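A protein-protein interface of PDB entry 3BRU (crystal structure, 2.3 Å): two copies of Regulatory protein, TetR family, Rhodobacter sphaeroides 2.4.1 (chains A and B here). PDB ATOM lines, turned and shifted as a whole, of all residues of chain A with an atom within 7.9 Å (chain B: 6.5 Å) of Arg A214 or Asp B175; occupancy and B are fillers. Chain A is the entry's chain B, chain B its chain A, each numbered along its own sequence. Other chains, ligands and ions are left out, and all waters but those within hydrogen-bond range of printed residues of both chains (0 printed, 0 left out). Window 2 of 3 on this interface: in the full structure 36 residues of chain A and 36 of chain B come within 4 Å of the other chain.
The guanidinium group (NH2) of Arg A214 lies within salt-bridge range of the side-chain carboxylate (OD1) of Asp B175 (3.4 Å). OD2 of Asp B177 is in salt-bridge range of NH2 of Arg A210 (3.7 Å). A ring nitrogen (NE2) of His B215 is in hydrogen-bond range of a ring nitrogen (NE2) of His A215 (3.4 Å).
NE2 of Gln B167 is in hydrogen-bond range of O of His B176 (2.9 Å). OG of Ser B173 sits close to N of Asp B175. NE2 of His B176 lies within hydrogen-bond range of O of His B215 (3.0 Å). A ring nitrogen (NE2) of His A176 sits at hydrogen-bond distance from the backbone carbonyl oxygen (O) of His A215.
Among the printed residues, pairs that only touch across the chains: Thr A211 with His B215 and Arg A214 with His B176.
Asp B175 touches just one residue of chain A: Arg A214. No residue of chain A comes within 4 Å of Ala B174. Of the printed residues of chain A, His B215 touches Thr A211 (3.1 Å) and His A215 (3.4 Å). Printed residues of chain A within 4 Å of His B176: Arg A214 (3.5 Å). Printed residues of chain A within 4 Å of Asp B177: Arg A210. Printed residues of chain B within 4 Å of Arg A210: Asp B177. Of the printed residues of chain B, His A215 touches His B215. Phe A216 touches none of the printed residues of chain B. The nearest residue of chain B that does not touch Arg A214 is His B215 (4.5 Å). The nearest residue of chain A that does not touch Asp B175 is Arg A210 (7.2 Å). The nearest printed residue of chain A that does not touch Asp B177 is Arg A214 (5.0 Å).
Printed residues of chain A that touch a printed residue of chain B: Arg A210, Thr A211, Arg A214 and His A215. Printed residues of chain B that touch a printed residue of chain A: Asp B175, His B176, Asp B177 and His B215. Along chain B the printed residues that touch a printed residue of chain A span positions 175 to 215. Among the printed residues, Asp or Glu carboxylates within 4 Å of a Lys or Arg side-chain nitrogen of the other chain: Arg A210 with Asp B177 (3.7 Å) and Arg A214 with Asp B175 (3.4 Å).
His A215 touches its own counterpart, His B215. Positions printed for both chains: 172, 176 and 215.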
ATOM      1  N   LEU A 105      28.567 -27.991 -19.811  1.00  0.00           N
ATOM      2  CA  LEU A 105      28.925 -26.693 -19.260  1.00  0.00           C
ATOM      3  C   LEU A 105      30.434 -26.548 -18.983  1.00  0.00           C
ATOM      4  O   LEU A 105      31.008 -25.477 -19.187  1.00  0.00           O
ATOM      5  CB  LEU A 105      28.087 -26.443 -17.994  1.00  0.00           C
ATOM      6  CG  LEU A 105      28.263 -25.113 -17.259  1.00  0.00           C
ATOM      7  CD1 LEU A 105      28.386 -23.878 -18.225  1.00  0.00           C
ATOM      8  CD2 LEU A 105      27.161 -24.916 -16.205  1.00  0.00           C
ATOM      9  N   LEU A 172      21.147 -27.045 -17.586  1.00  0.00           N
ATOM     10  CA  LEU A 172      20.415 -25.869 -17.978  1.00  0.00           C
ATOM     11  C   LEU A 172      18.939 -26.252 -17.948  1.00  0.00           C
ATOM     12  O   LEU A 172      18.566 -27.311 -18.469  1.00  0.00           O
ATOM     13  CB  LEU A 172      20.806 -25.458 -19.407  1.00  0.00           C
ATOM     14  CG  LEU A 172      20.081 -24.227 -20.012  1.00  0.00           C
ATOM     15  CD1 LEU A 172      20.364 -22.969 -19.212  1.00  0.00           C
ATOM     16  CD2 LEU A 172      20.396 -24.043 -21.506  1.00  0.00           C
ATOM     17  N   HIS A 176      14.667 -22.453 -20.787  1.00  0.00           N
ATOM     18  CA  HIS A 176      15.572 -21.659 -21.613  1.00  0.00           C
ATOM     19  C   HIS A 176      15.478 -22.114 -23.076  1.00  0.00           C
ATOM     20  O   HIS A 176      15.101 -23.264 -23.362  1.00  0.00           O
ATOM     21  CB  HIS A 176      17.018 -21.804 -21.114  1.00  0.00           C
ATOM     22  CG  HIS A 176      17.316 -21.011 -19.883  1.00  0.00           C
ATOM     23  ND1 HIS A 176      17.859 -19.741 -19.928  1.00  0.00           N
ATOM     24  CD2 HIS A 176      17.134 -21.293 -18.569  1.00  0.00           C
ATOM     25  CE1 HIS A 176      17.996 -19.275 -18.697  1.00  0.00           C
ATOM     26  NE2 HIS A 176      17.567 -20.200 -17.854  1.00  0.00           N
ATOM     27  N   PHE A 208      32.167 -11.177 -17.545  1.00  0.00           N
ATOM     28  CA  PHE A 208      31.191 -11.765 -18.467  1.00  0.00           C
ATOM     29  C   PHE A 208      30.841 -13.195 -18.082  1.00  0.00           C
ATOM     30  O   PHE A 208      29.664 -13.512 -17.902  1.00  0.00           O
ATOM     31  CB  PHE A 208      31.660 -11.782 -19.920  1.00  0.00           C
ATOM     32  CG  PHE A 208      30.758 -12.617 -20.813  1.00  0.00           C
ATOM     33  CD1 PHE A 208      29.459 -12.184 -21.126  1.00  0.00           C
ATOM     34  CD2 PHE A 208      31.191 -13.842 -21.323  1.00  0.00           C
ATOM     35  CE1 PHE A 208      28.607 -12.961 -21.935  1.00  0.00           C
ATOM     36  CE2 PHE A 208      30.375 -14.613 -22.137  1.00  0.00           C
ATOM     37  CZ  PHE A 208      29.068 -14.169 -22.446  1.00  0.00           C
ATOM     38  N   THR A 209      31.848 -14.059 -17.978  1.00  0.00           N
ATOM     39  CA  THR A 209      31.586 -15.464 -17.725  1.00  0.00           C
ATOM     40  C   THR A 209      31.017 -15.757 -16.328  1.00  0.00           C
ATOM     41  O   THR A 209      30.206 -16.660 -16.174  1.00  0.00           O
ATOM     42  CB  THR A 209      32.824 -16.371 -18.036  1.00  0.00           C
ATOM     43  OG1 THR A 209      33.861 -16.166 -17.062  1.00  0.00           O
ATOM     44  CG2 THR A 209      33.327 -16.157 -19.491  1.00  0.00           C
ATOM     45  N   ARG A 210      31.406 -14.988 -15.324  1.00  0.00           N
ATOM     46  CA  ARG A 210      30.860 -15.213 -14.006  1.00  0.00           C
ATOM     47  C   ARG A 210      29.352 -14.876 -13.952  1.00  0.00           C
ATOM     48  O   ARG A 210      28.562 -15.629 -13.377  1.00  0.00           O
ATOM     49  CB  ARG A 210      31.713 -14.543 -12.910  1.00  0.00           C
ATOM     50  CG  ARG A 210      30.954 -13.568 -11.979  1.00  0.00           C
ATOM     51  CD  ARG A 210      31.796 -13.216 -10.734  1.00  0.00           C
ATOM     52  NE  ARG A 210      31.012 -12.633  -9.623  1.00  0.00           N
ATOM     53  CZ  ARG A 210      31.328 -11.506  -8.958  1.00  0.00           C
ATOM     54  NH1 ARG A 210      32.420 -10.804  -9.292  1.00  0.00           N
ATOM     55  NH2 ARG A 210      30.559 -11.071  -7.950  1.00  0.00           N
ATOM     56  N   THR A 211      28.953 -13.788 -14.586  1.00  0.00           N
ATOM     57  CA  THR A 211      27.539 -13.392 -14.627  1.00  0.00           C
ATOM     58  C   THR A 211      26.704 -14.243 -15.604  1.00  0.00           C
ATOM     59  O   THR A 211      25.602 -14.654 -15.268  1.00  0.00           O
ATOM     60  CB  THR A 211      27.419 -11.900 -14.948  1.00  0.00           C
ATOM     61  OG1 THR A 211      27.899 -11.158 -13.823  1.00  0.00           O
ATOM     62  CG2 THR A 211      26.000 -11.491 -15.204  1.00  0.00           C
ATOM     63  N   PHE A 212      27.220 -14.496 -16.801  1.00  0.00           N
ATOM     64  CA  PHE A 212      26.507 -15.337 -17.735  1.00  0.00           C
ATOM     65  C   PHE A 212      26.303 -16.729 -17.146  1.00  0.00           C
ATOM     66  O   PHE A 212      25.335 -17.431 -17.468  1.00  0.00           O
ATOM     67  CB  PHE A 212      27.269 -15.466 -19.066  1.00  0.00           C
ATOM     68  CG  PHE A 212      26.428 -16.031 -20.185  1.00  0.00           C
ATOM     69  CD1 PHE A 212      25.621 -15.189 -20.960  1.00  0.00           C
ATOM     70  CD2 PHE A 212      26.434 -17.385 -20.462  1.00  0.00           C
ATOM     71  CE1 PHE A 212      24.848 -15.694 -21.991  1.00  0.00           C
ATOM     72  CE2 PHE A 212      25.633 -17.921 -21.494  1.00  0.00           C
ATOM     73  CZ  PHE A 212      24.835 -17.066 -22.257  1.00  0.00           C
ATOM     74  N   GLY A 213      27.250 -17.149 -16.318  1.00  0.00           N
ATOM     75  CA  GLY A 213      27.190 -18.490 -15.741  1.00  0.00           C
ATOM     76  C   GLY A 213      25.970 -18.698 -14.877  1.00  0.00           C
ATOM     77  O   GLY A 213      25.645 -19.814 -14.545  1.00  0.00           O
ATOM     78  N   ARG A 214      25.290 -17.617 -14.518  1.00  0.00           N
ATOM     79  CA  ARG A 214      24.159 -17.719 -13.618  1.00  0.00           C
ATOM     80  C   ARG A 214      22.870 -18.107 -14.335  1.00  0.00           C
ATOM     81  O   ARG A 214      21.893 -18.407 -13.676  1.00  0.00           O
ATOM     82  CB  ARG A 214      23.998 -16.432 -12.826  1.00  0.00           C
ATOM     83  CG  ARG A 214      25.119 -16.253 -11.840  1.00  0.00           C
ATOM     84  CD  ARG A 214      24.933 -15.029 -11.003  1.00  0.00           C
ATOM     85  NE  ARG A 214      23.793 -15.192 -10.094  1.00  0.00           N
ATOM     86  CZ  ARG A 214      23.717 -14.632  -8.892  1.00  0.00           C
ATOM     87  NH1 ARG A 214      24.722 -13.901  -8.440  1.00  0.00           N
ATOM     88  NH2 ARG A 214      22.645 -14.808  -8.144  1.00  0.00           N
ATOM     89  N   HIS A 215      22.881 -18.135 -15.666  1.00  0.00           N
ATOM     90  CA  HIS A 215      21.818 -18.784 -16.455  1.00  0.00           C
ATOM     91  C   HIS A 215      21.700 -20.297 -16.279  1.00  0.00           C
ATOM     92  O   HIS A 215      20.668 -20.872 -16.623  1.00  0.00           O
ATOM     93  CB  HIS A 215      21.998 -18.481 -17.939  1.00  0.00           C
ATOM     94  CG  HIS A 215      21.896 -17.024 -18.266  1.00  0.00           C
ATOM     95  ND1 HIS A 215      20.830 -16.243 -17.864  1.00  0.00           N
ATOM     96  CD2 HIS A 215      22.720 -16.201 -18.957  1.00  0.00           C
ATOM     97  CE1 HIS A 215      20.998 -15.009 -18.302  1.00  0.00           C
ATOM     98  NE2 HIS A 215      22.143 -14.955 -18.959  1.00  0.00           N
ATOM     99  N   PHE A 216      22.742 -20.937 -15.742  1.00  0.00           N
ATOM    100  CA  PHE A 216      22.769 -22.411 -15.499  1.00  0.00           C
ATOM    101  C   PHE A 216      22.351 -22.769 -14.093  1.00  0.00           C
ATOM    102  O   PHE A 216      22.414 -21.898 -13.226  1.00  0.00           O
ATOM    103  CB  PHE A 216      24.144 -22.940 -15.884  1.00  0.00           C
ATOM    104  CG  PHE A 216      24.509 -22.537 -17.275  1.00  0.00           C
ATOM    105  CD1 PHE A 216      24.009 -23.247 -18.369  1.00  0.00           C
ATOM    106  CD2 PHE A 216      25.233 -21.396 -17.506  1.00  0.00           C
ATOM    107  CE1 PHE A 216      24.290 -22.833 -19.660  1.00  0.00           C
ATOM    108  CE2 PHE A 216      25.531 -20.994 -18.785  1.00  0.00           C
ATOM    109  CZ  PHE A 216      25.052 -21.686 -19.861  1.00  0.00           C
ATOM    110  N   VAL A 217      21.863 -23.995 -13.871  1.00  0.00           N
ATOM    111  CA  VAL A 217      21.301 -24.379 -12.541  1.00  0.00           C
ATOM    112  C   VAL A 217      22.362 -24.507 -11.432  1.00  0.00           C
ATOM    113  O   VAL A 217      23.445 -25.037 -11.656  1.00  0.00           O
ATOM    114  CB  VAL A 217      20.272 -25.624 -12.554  1.00  0.00           C
ATOM    115  CG1 VAL A 217      19.685 -25.890 -13.946  1.00  0.00           C
ATOM    116  CG2 VAL A 217      20.866 -26.895 -11.985  1.00  0.00           C
ATOM    117  N   GLN B 167      17.530  -3.328  -5.953  1.00  0.00           N
ATOM    118  CA  GLN B 167      17.588  -4.214  -4.782  1.00  0.00           C
ATOM    119  C   GLN B 167      16.785  -3.697  -3.593  1.00  0.00           C
ATOM    120  O   GLN B 167      16.104  -4.468  -2.926  1.00  0.00           O
ATOM    121  CB  GLN B 167      19.030  -4.449  -4.348  1.00  0.00           C
ATOM    122  CG  GLN B 167      19.767  -5.377  -5.282  1.00  0.00           C
ATOM    123  CD  GLN B 167      21.124  -5.773  -4.773  1.00  0.00           C
ATOM    124  OE1 GLN B 167      21.921  -4.928  -4.383  1.00  0.00           O
ATOM    125  NE2 GLN B 167      21.409  -7.063  -4.800  1.00  0.00           N
ATOM    126  N   LEU B 172      15.365  -6.714  -7.792  1.00  0.00           N
ATOM    127  CA  LEU B 172      16.551  -7.520  -7.987  1.00  0.00           C
ATOM    128  C   LEU B 172      16.780  -8.284  -6.685  1.00  0.00           C
ATOM    129  O   LEU B 172      16.501  -7.763  -5.604  1.00  0.00           O
ATOM    130  CB  LEU B 172      17.746  -6.598  -8.228  1.00  0.00           C
ATOM    131  CG  LEU B 172      18.774  -6.807  -9.340  1.00  0.00           C
ATOM    132  CD1 LEU B 172      20.092  -6.263  -8.887  1.00  0.00           C
ATOM    133  CD2 LEU B 172      18.937  -8.262  -9.809  1.00  0.00           C
ATOM    134  N   SER B 173      17.277  -9.515  -6.768  1.00  0.00           N
ATOM    135  CA  SER B 173      17.431 -10.306  -5.552  1.00  0.00           C
ATOM    136  C   SER B 173      18.668  -9.830  -4.804  1.00  0.00           C
ATOM    137  O   SER B 173      19.643  -9.411  -5.437  1.00  0.00           O
ATOM    138  CB  SER B 173      17.464 -11.820  -5.854  1.00  0.00           C
ATOM    139  OG  SER B 173      18.772 -12.316  -6.089  1.00  0.00           O
ATOM    140  N   ALA B 174      18.613  -9.872  -3.470  1.00  0.00           N
ATOM    141  CA  ALA B 174      19.740  -9.486  -2.608  1.00  0.00           C
ATOM    142  C   ALA B 174      20.994 -10.280  -2.957  1.00  0.00           C
ATOM    143  O   ALA B 174      22.101  -9.876  -2.649  1.00  0.00           O
ATOM    144  CB  ALA B 174      19.381  -9.685  -1.150  1.00  0.00           C
ATOM    145  N   ASP B 175      20.783 -11.403  -3.622  1.00  0.00           N
ATOM    146  CA  ASP B 175      21.817 -12.279  -4.147  1.00  0.00           C
ATOM    147  C   ASP B 175      22.878 -11.636  -5.078  1.00  0.00           C
ATOM    148  O   ASP B 175      24.085 -11.894  -4.935  1.00  0.00           O
ATOM    149  CB  ASP B 175      21.096 -13.365  -4.925  1.00  0.00           C
ATOM    150  CG  ASP B 175      21.758 -14.672  -4.817  1.00  0.00           C
ATOM    151  OD1 ASP B 175      21.126 -15.677  -5.199  1.00  0.00           O
ATOM    152  OD2 ASP B 175      22.905 -14.705  -4.337  1.00  0.00           O
ATOM    153  N   HIS B 176      22.417 -10.829  -6.031  1.00  0.00           N
ATOM    154  CA  HIS B 176      23.250 -10.237  -7.084  1.00  0.00           C
ATOM    155  C   HIS B 176      24.203  -9.133  -6.631  1.00  0.00           C
ATOM    156  O   HIS B 176      23.855  -8.327  -5.760  1.00  0.00           O
ATOM    157  CB  HIS B 176      22.343  -9.687  -8.183  1.00  0.00           C
ATOM    158  CG  HIS B 176      21.748 -10.751  -9.037  1.00  0.00           C
ATOM    159  ND1 HIS B 176      22.462 -11.382 -10.032  1.00  0.00           N
ATOM    160  CD2 HIS B 176      20.526 -11.333  -9.019  1.00  0.00           C
ATOM    161  CE1 HIS B 176      21.702 -12.305 -10.600  1.00  0.00           C
ATOM    162  NE2 HIS B 176      20.525 -12.300  -9.998  1.00  0.00           N
ATOM    163  N   ASP B 177      25.396  -9.093  -7.227  1.00  0.00           N
ATOM    164  CA  ASP B 177      26.304  -7.956  -7.046  1.00  0.00           C
ATOM    165  C   ASP B 177      25.958  -6.855  -8.078  1.00  0.00           C
ATOM    166  O   ASP B 177      26.069  -7.089  -9.290  1.00  0.00           O
ATOM    167  CB  ASP B 177      27.781  -8.405  -7.140  1.00  0.00           C
ATOM    168  CG  ASP B 177      28.792  -7.224  -7.033  1.00  0.00           C
ATOM    169  OD1 ASP B 177      28.385  -6.073  -6.745  1.00  0.00           O
ATOM    170  OD2 ASP B 177      30.018  -7.446  -7.243  1.00  0.00           O
ATOM    171  N   HIS B 215      18.173 -12.223 -15.390  1.00  0.00           N
ATOM    172  CA  HIS B 215      18.946 -11.976 -14.167  1.00  0.00           C
ATOM    173  C   HIS B 215      18.099 -11.311 -13.079  1.00  0.00           C
ATOM    174  O   HIS B 215      18.505 -11.283 -11.935  1.00  0.00           O
ATOM    175  CB  HIS B 215      20.189 -11.115 -14.438  1.00  0.00           C
ATOM    176  CG  HIS B 215      21.246 -11.794 -15.258  1.00  0.00           C
ATOM    177  ND1 HIS B 215      21.935 -12.904 -14.818  1.00  0.00           N
ATOM    178  CD2 HIS B 215      21.761 -11.494 -16.478  1.00  0.00           C
ATOM    179  CE1 HIS B 215      22.821 -13.262 -15.734  1.00  0.00           C
ATOM    180  NE2 HIS B 215      22.739 -12.422 -16.750  1.00  0.00           N
